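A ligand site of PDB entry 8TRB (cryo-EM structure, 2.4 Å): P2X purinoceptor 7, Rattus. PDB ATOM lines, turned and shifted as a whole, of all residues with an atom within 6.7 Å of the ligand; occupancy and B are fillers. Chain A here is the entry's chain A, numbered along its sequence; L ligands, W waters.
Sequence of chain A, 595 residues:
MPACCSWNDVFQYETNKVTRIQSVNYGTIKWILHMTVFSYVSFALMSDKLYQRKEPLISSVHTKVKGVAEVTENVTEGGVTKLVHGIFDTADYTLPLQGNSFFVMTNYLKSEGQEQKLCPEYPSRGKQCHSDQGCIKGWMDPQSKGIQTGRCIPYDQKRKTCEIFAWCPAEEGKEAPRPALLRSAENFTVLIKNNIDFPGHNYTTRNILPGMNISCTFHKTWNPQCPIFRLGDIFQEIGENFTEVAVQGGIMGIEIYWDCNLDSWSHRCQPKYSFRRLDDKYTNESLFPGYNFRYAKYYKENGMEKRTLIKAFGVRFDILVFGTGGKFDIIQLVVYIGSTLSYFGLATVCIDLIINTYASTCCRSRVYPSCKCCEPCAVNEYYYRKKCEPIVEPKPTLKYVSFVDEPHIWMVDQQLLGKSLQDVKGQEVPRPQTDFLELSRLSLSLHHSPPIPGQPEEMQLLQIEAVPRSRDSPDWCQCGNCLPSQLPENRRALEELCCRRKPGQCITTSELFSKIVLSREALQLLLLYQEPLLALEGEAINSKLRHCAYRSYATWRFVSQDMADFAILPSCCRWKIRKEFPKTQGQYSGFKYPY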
ATOM      1  N   GLU A 495       3.228  17.378 -12.210  1.00  0.00           N
ATOM      2  CA  GLU A 495       3.239  18.644 -12.928  1.00  0.00           C
ATOM      3  C   GLU A 495       3.662  18.501 -14.378  1.00  0.00           C
ATOM      4  O   GLU A 495       3.703  19.501 -15.102  1.00  0.00           O
ATOM      5  CB  GLU A 495       4.162  19.638 -12.224  1.00  0.00           C
ATOM      6  CG  GLU A 495       3.672  20.076 -10.860  1.00  0.00           C
ATOM      7  CD  GLU A 495       4.345  21.339 -10.374  1.00  0.00           C
ATOM      8  OE1 GLU A 495       5.253  21.833 -11.070  1.00  0.00           O
ATOM      9  OE2 GLU A 495       3.965  21.835  -9.295  1.00  0.00           O
ATOM     10  N   SER A 543       1.521  35.221  -3.167  1.00  0.00           N
ATOM     11  CA  SER A 543       1.013  33.863  -3.017  1.00  0.00           C
ATOM     12  C   SER A 543      -0.503  33.828  -3.180  1.00  0.00           C
ATOM     13  O   SER A 543      -1.048  32.913  -3.804  1.00  0.00           O
ATOM     14  CB  SER A 543       1.420  33.313  -1.646  1.00  0.00           C
ATOM     15  OG  SER A 543       1.421  31.901  -1.631  1.00  0.00           O
ATOM     16  N   ARG A 546      -1.371  34.162  -6.775  1.00  0.00           N
ATOM     17  CA  ARG A 546      -1.106  32.905  -7.463  1.00  0.00           C
ATOM     18  C   ARG A 546      -2.224  31.900  -7.217  1.00  0.00           C
ATOM     19  O   ARG A 546      -2.685  31.233  -8.148  1.00  0.00           O
ATOM     20  CB  ARG A 546       0.220  32.327  -6.979  1.00  0.00           C
ATOM     21  CG  ARG A 546       1.381  32.584  -7.913  1.00  0.00           C
ATOM     22  CD  ARG A 546       2.484  31.592  -7.678  1.00  0.00           C
ATOM     23  NE  ARG A 546       2.664  31.292  -6.257  1.00  0.00           N
ATOM     24  CZ  ARG A 546       3.281  32.088  -5.392  1.00  0.00           C
ATOM     25  NH1 ARG A 546       3.790  33.243  -5.803  1.00  0.00           N
ATOM     26  NH2 ARG A 546       3.386  31.726  -4.125  1.00  0.00           N
ATOM     27  N   HIS A 547      -2.656  31.786  -5.968  1.00  0.00           N
ATOM     28  CA  HIS A 547      -3.737  30.867  -5.646  1.00  0.00           C
ATOM     29  C   HIS A 547      -5.008  31.228  -6.384  1.00  0.00           C
ATOM     30  O   HIS A 547      -5.701  30.357  -6.930  1.00  0.00           O
ATOM     31  CB  HIS A 547      -3.973  30.846  -4.131  1.00  0.00           C
ATOM     32  CG  HIS A 547      -2.755  30.494  -3.331  1.00  0.00           C
ATOM     33  ND1 HIS A 547      -1.566  30.126  -3.914  1.00  0.00           N
ATOM     34  CD2 HIS A 547      -2.561  30.445  -1.994  1.00  0.00           C
ATOM     35  CE1 HIS A 547      -0.675  29.877  -2.970  1.00  0.00           C
ATOM     36  NE2 HIS A 547      -1.261  30.052  -1.794  1.00  0.00           N
ATOM     37  N   TYR A 550      -4.673  30.339 -10.079  1.00  0.00           N
ATOM     38  CA  TYR A 550      -4.900  28.903 -10.246  1.00  0.00           C
ATOM     39  C   TYR A 550      -6.384  28.587 -10.193  1.00  0.00           C
ATOM     40  O   TYR A 550      -6.902  27.842 -11.041  1.00  0.00           O
ATOM     41  CB  TYR A 550      -4.158  28.115  -9.177  1.00  0.00           C
ATOM     42  CG  TYR A 550      -2.658  28.224  -9.200  1.00  0.00           C
ATOM     43  CD1 TYR A 550      -1.962  28.438 -10.385  1.00  0.00           C
ATOM     44  CD2 TYR A 550      -1.924  28.103  -8.029  1.00  0.00           C
ATOM     45  CE1 TYR A 550      -0.594  28.529 -10.398  1.00  0.00           C
ATOM     46  CE2 TYR A 550      -0.556  28.194  -8.041  1.00  0.00           C
ATOM     47  CZ  TYR A 550       0.106  28.408  -9.214  1.00  0.00           C
ATOM     48  OH  TYR A 550       1.472  28.508  -9.206  1.00  0.00           O
ATOM     49  N   ARG A 551      -7.083  29.129  -9.200  1.00  0.00           N
ATOM     50  CA  ARG A 551      -8.517  28.887  -9.085  1.00  0.00           C
ATOM     51  C   ARG A 551      -9.259  29.397 -10.308  1.00  0.00           C
ATOM     52  O   ARG A 551     -10.209  28.756 -10.777  1.00  0.00           O
ATOM     53  CB  ARG A 551      -9.066  29.540  -7.813  1.00  0.00           C
ATOM     54  CG  ARG A 551      -9.040  28.637  -6.590  1.00  0.00           C
ATOM     55  CD  ARG A 551      -8.759  29.413  -5.310  1.00  0.00           C
ATOM     56  NE  ARG A 551      -7.746  28.746  -4.481  1.00  0.00           N
ATOM     57  CZ  ARG A 551      -7.048  29.339  -3.524  1.00  0.00           C
ATOM     58  NH1 ARG A 551      -7.226  30.630  -3.259  1.00  0.00           N
ATOM     59  NH2 ARG A 551      -6.164  28.651  -2.827  1.00  0.00           N
ATOM     60  N   ALA A 554      -8.657  27.071 -13.230  1.00  0.00           N
ATOM     61  CA  ALA A 554      -9.357  25.815 -12.986  1.00  0.00           C
ATOM     62  C   ALA A 554     -10.849  25.974 -13.180  1.00  0.00           C
ATOM     63  O   ALA A 554     -11.506  25.084 -13.725  1.00  0.00           O
ATOM     64  CB  ALA A 554      -9.050  25.325 -11.581  1.00  0.00           C
ATOM     65  N   MET A 563     -14.694  19.474  -9.857  1.00  0.00           N
ATOM     66  CA  MET A 563     -13.603  19.121 -10.757  1.00  0.00           C
ATOM     67  C   MET A 563     -12.460  20.123 -10.673  1.00  0.00           C
ATOM     68  O   MET A 563     -11.293  19.739 -10.818  1.00  0.00           O
ATOM     69  CB  MET A 563     -14.105  19.018 -12.194  1.00  0.00           C
ATOM     70  CG  MET A 563     -14.884  17.747 -12.474  1.00  0.00           C
ATOM     71  SD  MET A 563     -14.949  17.279 -14.201  1.00  0.00           S
ATOM     72  CE  MET A 563     -15.543  18.797 -14.934  1.00  0.00           C
ATOM     73  N   ALA A 564     -12.763  21.406 -10.446  1.00  0.00           N
ATOM     74  CA  ALA A 564     -11.724  22.413 -10.346  1.00  0.00           C
ATOM     75  C   ALA A 564     -10.855  22.217  -9.111  1.00  0.00           C
ATOM     76  O   ALA A 564      -9.672  22.562  -9.122  1.00  0.00           O
ATOM     77  CB  ALA A 564     -12.343  23.807 -10.331  1.00  0.00           C
ATOM     78  N   ASP A 565     -11.429  21.675  -8.039  1.00  0.00           N
ATOM     79  CA  ASP A 565     -10.670  21.480  -6.805  1.00  0.00           C
ATOM     80  C   ASP A 565      -9.551  20.468  -6.986  1.00  0.00           C
ATOM     81  O   ASP A 565      -8.478  20.611  -6.396  1.00  0.00           O
ATOM     82  CB  ASP A 565     -11.609  21.070  -5.680  1.00  0.00           C
ATOM     83  CG  ASP A 565     -12.429  22.227  -5.153  1.00  0.00           C
ATOM     84  OD1 ASP A 565     -12.236  23.367  -5.616  1.00  0.00           O
ATOM     85  OD2 ASP A 565     -13.276  21.996  -4.256  1.00  0.00           O
ATOM     86  N   PHE A 566      -9.787  19.434  -7.787  1.00  0.00           N
ATOM     87  CA  PHE A 566      -8.767  18.440  -8.078  1.00  0.00           C
ATOM     88  C   PHE A 566      -8.199  18.576  -9.492  1.00  0.00           C
ATOM     89  O   PHE A 566      -7.546  17.646  -9.975  1.00  0.00           O
ATOM     90  CB  PHE A 566      -9.304  17.022  -7.880  1.00  0.00           C
ATOM     91  CG  PHE A 566      -9.839  16.770  -6.517  1.00  0.00           C
ATOM     92  CD1 PHE A 566     -11.119  17.157  -6.177  1.00  0.00           C
ATOM     93  CD2 PHE A 566      -9.083  16.102  -5.579  1.00  0.00           C
ATOM     94  CE1 PHE A 566     -11.613  16.910  -4.918  1.00  0.00           C
ATOM     95  CE2 PHE A 566      -9.564  15.857  -4.326  1.00  0.00           C
ATOM     96  CZ  PHE A 566     -10.835  16.260  -3.992  1.00  0.00           C
ATOM     97  N   ALA A 567      -8.426  19.700 -10.143  1.00  0.00           N
ATOM     98  CA  ALA A 567      -7.831  19.931 -11.447  1.00  0.00           C
ATOM     99  C   ALA A 567      -6.332  20.096 -11.318  1.00  0.00           C
ATOM    100  O   ALA A 567      -5.809  20.387 -10.238  1.00  0.00           O
ATOM    101  CB  ALA A 567      -8.443  21.158 -12.108  1.00  0.00           C
ATOM    102  N   ILE A 568      -5.626  19.895 -12.424  1.00  0.00           N
ATOM    103  CA  ILE A 568      -4.187  20.057 -12.491  1.00  0.00           C
ATOM    104  C   ILE A 568      -3.883  21.063 -13.588  1.00  0.00           C
ATOM    105  O   ILE A 568      -4.300  20.880 -14.733  1.00  0.00           O
ATOM    106  CB  ILE A 568      -3.462  18.734 -12.737  1.00  0.00           C
ATOM    107  CG1 ILE A 568      -3.939  17.654 -11.753  1.00  0.00           C
ATOM    108  CG2 ILE A 568      -1.967  18.929 -12.602  1.00  0.00           C
ATOM    109  CD1 ILE A 568      -3.655  17.963 -10.325  1.00  0.00           C
ATOM    110  N   LEU A 569      -3.166  22.107 -13.233  1.00  0.00           N
ATOM    111  CA  LEU A 569      -2.819  23.118 -14.206  1.00  0.00           C
ATOM    112  C   LEU A 569      -1.680  22.631 -15.094  1.00  0.00           C
ATOM    113  O   LEU A 569      -0.798  21.896 -14.647  1.00  0.00           O
ATOM    114  CB  LEU A 569      -2.401  24.401 -13.498  1.00  0.00           C
ATOM    115  CG  LEU A 569      -3.475  25.467 -13.335  1.00  0.00           C
ATOM    116  CD1 LEU A 569      -4.323  25.197 -12.112  1.00  0.00           C
ATOM    117  CD2 LEU A 569      -2.825  26.817 -13.264  1.00  0.00           C
ATOM    118  N   PRO A 570      -1.668  23.038 -16.360  1.00  0.00           N
ATOM    119  CA  PRO A 570      -0.513  22.729 -17.217  1.00  0.00           C
ATOM    120  C   PRO A 570       0.727  23.475 -16.751  1.00  0.00           C
ATOM    121  O   PRO A 570       0.643  24.523 -16.106  1.00  0.00           O
ATOM    122  CB  PRO A 570      -0.967  23.192 -18.594  1.00  0.00           C
ATOM    123  CG  PRO A 570      -2.423  23.330 -18.513  1.00  0.00           C
ATOM    124  CD  PRO A 570      -2.736  23.692 -17.122  1.00  0.00           C
ATOM    125  N   ARG A 574       0.918  27.262 -15.412  1.00  0.00           N
ATOM    126  CA  ARG A 574       1.429  27.329 -14.046  1.00  0.00           C
ATOM    127  C   ARG A 574       2.625  28.259 -13.944  1.00  0.00           C
ATOM    128  O   ARG A 574       2.682  29.130 -13.071  1.00  0.00           O
ATOM    129  CB  ARG A 574       1.788  25.930 -13.569  1.00  0.00           C
ATOM    130  CG  ARG A 574       2.405  25.856 -12.189  1.00  0.00           C
ATOM    131  CD  ARG A 574       2.967  24.489 -11.937  1.00  0.00           C
ATOM    132  NE  ARG A 574       2.048  23.432 -12.333  1.00  0.00           N
ATOM    133  CZ  ARG A 574       1.085  22.956 -11.555  1.00  0.00           C
ATOM    134  NH1 ARG A 574       0.894  23.432 -10.335  1.00  0.00           N
ATOM    135  NH2 ARG A 574       0.295  21.984 -12.009  1.00  0.00           N
ATOM    136  N   ARG A 578       3.255  31.820 -12.162  1.00  0.00           N
ATOM    137  CA  ARG A 578       4.282  31.933 -11.144  1.00  0.00           C
ATOM    138  C   ARG A 578       5.293  33.019 -11.455  1.00  0.00           C
ATOM    139  O   ARG A 578       5.854  33.617 -10.525  1.00  0.00           O
ATOM    140  CB  ARG A 578       4.976  30.584 -10.957  1.00  0.00           C
ATOM    141  CG  ARG A 578       4.157  29.640 -10.105  1.00  0.00           C
ATOM    142  CD  ARG A 578       4.738  28.243 -10.006  1.00  0.00           C
ATOM    143  NE  ARG A 578       4.038  27.461  -8.996  1.00  0.00           N
ATOM    144  CZ  ARG A 578       4.163  26.151  -8.843  1.00  0.00           C
ATOM    145  NH1 ARG A 578       4.969  25.464  -9.636  1.00  0.00           N
ATOM    146  NH2 ARG A 578       3.477  25.519  -7.894  1.00  0.00           N
ATOM    147  N   LYS A 583       7.686  34.080  -6.535  1.00  0.00           N
ATOM    148  CA  LYS A 583       7.964  33.840  -5.132  1.00  0.00           C
ATOM    149  C   LYS A 583       9.413  34.263  -4.846  1.00  0.00           C
ATOM    150  O   LYS A 583      10.324  33.903  -5.600  1.00  0.00           O
ATOM    151  CB  LYS A 583       7.748  32.371  -4.771  1.00  0.00           C
ATOM    152  CG  LYS A 583       8.237  31.983  -3.403  1.00  0.00           C
ATOM    153  CD  LYS A 583       7.585  30.686  -2.938  1.00  0.00           C
ATOM    154  CE  LYS A 583       6.738  30.889  -1.703  1.00  0.00           C
ATOM    155  NZ  LYS A 583       6.701  29.670  -0.854  1.00  0.00           N
ATOM    156  N   GLY A 586      11.484  31.269  -1.592  1.00  0.00           N
ATOM    157  CA  GLY A 586      10.869  30.006  -1.225  1.00  0.00           C
ATOM    158  C   GLY A 586      10.770  29.089  -2.421  1.00  0.00           C
ATOM    159  O   GLY A 586      11.161  29.430  -3.543  1.00  0.00           O
ATOM    160  N   GLN A 587      10.226  27.897  -2.164  1.00  0.00           N
ATOM    161  CA  GLN A 587      10.017  26.886  -3.188  1.00  0.00           C
ATOM    162  C   GLN A 587       8.530  26.607  -3.306  1.00  0.00           C
ATOM    163  O   GLN A 587       7.848  26.381  -2.298  1.00  0.00           O
ATOM    164  CB  GLN A 587      10.772  25.601  -2.863  1.00  0.00           C
ATOM    165  CG  GLN A 587      10.747  24.561  -3.962  1.00  0.00           C
ATOM    166  CD  GLN A 587      11.933  24.670  -4.893  1.00  0.00           C
ATOM    167  OE1 GLN A 587      12.696  25.634  -4.854  1.00  0.00           O
ATOM    168  NE2 GLN A 587      12.109  23.670  -5.759  1.00  0.00           N
ATOM    169  N   TYR A 588       8.015  26.616  -4.535  1.00  0.00           N
ATOM    170  CA  TYR A 588       6.599  26.349  -4.759  1.00  0.00           C
ATOM    171  C   TYR A 588       6.240  24.934  -4.323  1.00  0.00           C
ATOM    172  O   TYR A 588       6.966  23.975  -4.609  1.00  0.00           O
ATOM    173  CB  TYR A 588       6.251  26.547  -6.236  1.00  0.00           C
ATOM    174  CG  TYR A 588       6.542  27.926  -6.758  1.00  0.00           C
ATOM    175  CD1 TYR A 588       5.797  29.014  -6.342  1.00  0.00           C
ATOM    176  CD2 TYR A 588       7.546  28.143  -7.677  1.00  0.00           C
ATOM    177  CE1 TYR A 588       6.049  30.285  -6.824  1.00  0.00           C
ATOM    178  CE2 TYR A 588       7.810  29.401  -8.173  1.00  0.00           C
ATOM    179  CZ  TYR A 588       7.055  30.467  -7.737  1.00  0.00           C
ATOM    180  OH  TYR A 588       7.323  31.727  -8.223  1.00  0.00           O
ATOM    181  N   SER A 589       5.110  24.808  -3.639  1.00  0.00           N
ATOM    182  CA  SER A 589       4.666  23.513  -3.122  1.00  0.00           C
ATOM    183  C   SER A 589       3.794  22.745  -4.115  1.00  0.00           C
ATOM    184  O   SER A 589       3.752  21.511  -4.059  1.00  0.00           O
ATOM    185  CB  SER A 589       3.896  23.716  -1.817  1.00  0.00           C
ATOM    186  OG  SER A 589       3.083  24.865  -1.882  1.00  0.00           O
ATOM    187  N   GLY A 590       3.114  23.438  -5.011  1.00  0.00           N
ATOM    188  CA  GLY A 590       2.294  22.786  -6.007  1.00  0.00           C
ATOM    189  C   GLY A 590       0.942  22.345  -5.483  1.00  0.00           C
ATOM    190  O   GLY A 590       0.471  22.765  -4.417  1.00  0.00           O
ATOM    191  N   PHE A 591       0.301  21.487  -6.270  1.00  0.00           N
ATOM    192  CA  PHE A 591      -1.012  20.976  -5.910  1.00  0.00           C
ATOM    193  C   PHE A 591      -0.943  20.110  -4.657  1.00  0.00           C
ATOM    194  O   PHE A 591      -0.019  19.323  -4.466  1.00  0.00           O
ATOM    195  CB  PHE A 591      -1.595  20.167  -7.068  1.00  0.00           C
ATOM    196  CG  PHE A 591      -2.946  19.586  -6.776  1.00  0.00           C
ATOM    197  CD1 PHE A 591      -4.047  20.415  -6.626  1.00  0.00           C
ATOM    198  CD2 PHE A 591      -3.123  18.221  -6.661  1.00  0.00           C
ATOM    199  CE1 PHE A 591      -5.283  19.889  -6.367  1.00  0.00           C
ATOM    200  CE2 PHE A 591      -4.367  17.701  -6.401  1.00  0.00           C
ATOM    201  CZ  PHE A 591      -5.439  18.537  -6.252  1.00  0.00           C
ATOM    202  N   LYS A 592      -1.955  20.266  -3.797  1.00  0.00           N
ATOM    203  CA  LYS A 592      -2.072  19.478  -2.579  1.00  0.00           C
ATOM    204  C   LYS A 592      -3.492  18.940  -2.445  1.00  0.00           C
ATOM    205  O   LYS A 592      -4.449  19.566  -2.904  1.00  0.00           O
ATOM    206  CB  LYS A 592      -1.717  20.306  -1.338  1.00  0.00           C
ATOM    207  CG  LYS A 592      -2.239  21.738  -1.391  1.00  0.00           C
ATOM    208  CD  LYS A 592      -1.707  22.607  -0.248  1.00  0.00           C
ATOM    209  CE  LYS A 592      -0.186  22.571  -0.126  1.00  0.00           C
ATOM    210  NZ  LYS A 592       0.492  22.863  -1.410  1.00  0.00           N
ATOM    211  N   TYR A 593      -3.609  17.783  -1.810  1.00  0.00           N
ATOM    212  CA  TYR A 593      -4.904  17.137  -1.622  1.00  0.00           C
ATOM    213  C   TYR A 593      -5.740  17.931  -0.624  1.00  0.00           C
ATOM    214  O   TYR A 593      -5.303  18.105   0.526  1.00  0.00           O
ATOM    215  CB  TYR A 593      -4.677  15.720  -1.134  1.00  0.00           C
ATOM    216  CG  TYR A 593      -5.925  14.894  -0.956  1.00  0.00           C
ATOM    217  CD1 TYR A 593      -6.924  14.892  -1.912  1.00  0.00           C
ATOM    218  CD2 TYR A 593      -6.113  14.106   0.169  1.00  0.00           C
ATOM    219  CE1 TYR A 593      -8.065  14.142  -1.759  1.00  0.00           C
ATOM    220  CE2 TYR A 593      -7.243  13.346   0.342  1.00  0.00           C
ATOM    221  CZ  TYR A 593      -8.221  13.363  -0.627  1.00  0.00           C
ATOM    222  OH  TYR A 593      -9.366  12.621  -0.462  1.00  0.00           O
ATOM    223  N   PRO A 594      -6.921  18.414  -0.998  1.00  0.00           N
ATOM    224  CA  PRO A 594      -7.723  19.176  -0.028  1.00  0.00           C
ATOM    225  C   PRO A 594      -8.093  18.386   1.220  1.00  0.00           C
ATOM    226  O   PRO A 594      -8.136  18.958   2.319  1.00  0.00           O
ATOM    227  CB  PRO A 594      -8.959  19.574  -0.832  1.00  0.00           C
ATOM    228  CG  PRO A 594      -8.545  19.484  -2.257  1.00  0.00           C
ATOM    229  CD  PRO A 594      -7.552  18.394  -2.329  1.00  0.00           C
HETATM  230  P1  LIG L   1       3.225  28.025  -2.163  1.00  0.00           P
HETATM  231  O1  LIG L   1       3.325  29.504  -1.925  1.00  0.00           O
HETATM  232  O2  LIG L   1       2.091  27.491  -1.318  1.00  0.00           O
HETATM  233  O3  LIG L   1       4.500  27.374  -1.687  1.00  0.00           O
HETATM  234  O4  LIG L   1       3.054  27.712  -3.731  1.00  0.00           O
HETATM  235  P2  LIG L   1       1.667  27.435  -4.500  1.00  0.00           P
HETATM  236  O5  LIG L   1       1.288  28.613  -5.335  1.00  0.00           O
HETATM  237  O6  LIG L   1       1.769  26.242  -5.393  1.00  0.00           O
HETATM  238  O7  LIG L   1       0.534  27.215  -3.389  1.00  0.00           O
HETATM  239  C1  LIG L   1      -0.143  25.984  -3.170  1.00  0.00           C
HETATM  240  C2  LIG L   1      -1.633  26.201  -3.313  1.00  0.00           C
HETATM  241  O8  LIG L   1      -1.974  26.444  -4.682  1.00  0.00           O
HETATM  242  C3  LIG L   1      -2.361  24.958  -2.853  1.00  0.00           C
HETATM  243  O9  LIG L   1      -3.353  25.267  -1.872  1.00  0.00           O
HETATM  244  C4  LIG L   1      -2.984  24.370  -4.091  1.00  0.00           C
HETATM  245  O10 LIG L   1      -4.341  23.964  -3.858  1.00  0.00           O
HETATM  246  C5  LIG L   1      -2.903  25.465  -5.136  1.00  0.00           C
HETATM  247  N1  LIG L   1      -2.442  24.815  -6.375  1.00  0.00           N
HETATM  248  C6  LIG L   1      -1.171  24.748  -6.784  1.00  0.00           C
HETATM  249  N2  LIG L   1      -1.090  24.052  -7.946  1.00  0.00           N
HETATM  250  C7  LIG L   1      -2.331  23.658  -8.262  1.00  0.00           C
HETATM  251  C8  LIG L   1      -2.950  22.899  -9.353  1.00  0.00           C
HETATM  252  O11 LIG L   1      -2.239  22.453 -10.252  1.00  0.00           O
HETATM  253  N3  LIG L   1      -4.264  22.689  -9.345  1.00  0.00           N
HETATM  254  C9  LIG L   1      -5.042  23.171  -8.363  1.00  0.00           C
HETATM  255  N4  LIG L   1      -6.368  22.912  -8.427  1.00  0.00           N
HETATM  256  N5  LIG L   1      -4.548  23.885  -7.313  1.00  0.00           N
HETATM  257  C10 LIG L   1      -3.220  24.156  -7.221  1.00  0.00           C
HETATM  258  O   HOH W   1      -7.746  22.900  -5.380  1.00  0.00           O
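Water W1 lies within hydrogen-bond range of the backbone carbonyl oxygen (O) of Asp 565 (2.6 Å) and a nitrogen (N4) of the ligand (3.3 Å).
N of Ser 589 is in hydrogen-bond range of O3 of the ligand (3.3 Å).
O2 of the ligand lies within hydrogen-bond range of OG of Ser 589 (2.9 Å).
O of Ala 567 is in hydrogen-bond range of N3 of the ligand (2.9 Å).
The side-chain hydroxyl (OG) of Ser 543 is in hydrogen-bond range of an oxygen (O1) of the ligand (3.1 Å).
An oxygen (O6) of the ligand is in salt-bridge range of the guanidinium group (NH2) of Arg 578 (3.1 Å).
The guanidinium group (NH2) of Arg 574 lies within hydrogen-bond range of an oxygen (O11) of the ligand, at 3.1 Å.
An oxygen (O1) of the ligand is in salt-bridge range of the guanidinium group (NH2) of Arg 546 (3.1 Å).
O6 of the ligand is in hydrogen-bond range of N of Gly 590 (3.1 Å).
N of Leu 569 sits at hydrogen-bond distance from O11 of the ligand (3.1 Å).
The side-chain amino group (NZ) of Lys 583 lies within salt-bridge range of an oxygen (O3) of the ligand (3.3 Å).
The backbone NH of Phe 591 sits at hydrogen-bond distance from a nitrogen (N2) of the ligand (3.4 Å).
The backbone carbonyl oxygen (O) of Ala 564 lies within hydrogen-bond range of a nitrogen (N4) of the ligand, at 3.4 Å.
OG of Ser 589 sits at hydrogen-bond distance from NZ of Lys 592 (3.3 Å).
The side-chain hydroxyl (OG) of Ser 543 is in hydrogen-bond range of the guanidinium group (NH2) of Arg 546 (3.2 Å).
NE of Arg 578 sits at hydrogen-bond distance from OH of Tyr 550.
O of Arg 578 is in hydrogen-bond range of OH of Tyr 588, 3.3 Å away.
The side-chain carboxylate of Glu 495 lies within salt-bridge range of the guanidinium group of Arg 578.
The guanidinium group of Arg 574 is in hydrogen-bond range of the backbone carbonyl oxygen of Leu 569, at 2.9 Å.
The side-chain carboxylate (OE2) of Glu 495 lies within salt-bridge range of the guanidinium group (NH1) of Arg 574 (3.6 Å).
O of Gly 590 lies within hydrogen-bond range of NZ of Lys 592 (3.0 Å).
Merely in contact with the ligand: His 547 (3.0 Å), Tyr 550 (3.3 Å), Asp 565 (3.7 Å), Ile 568 (3.8 Å), Gln 587 (3.5 Å), Tyr 588 (3.9 Å) and Lys 592 (3.5 Å).
Of the 27 residues printed, 18 come within 4 Å of the ligand.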
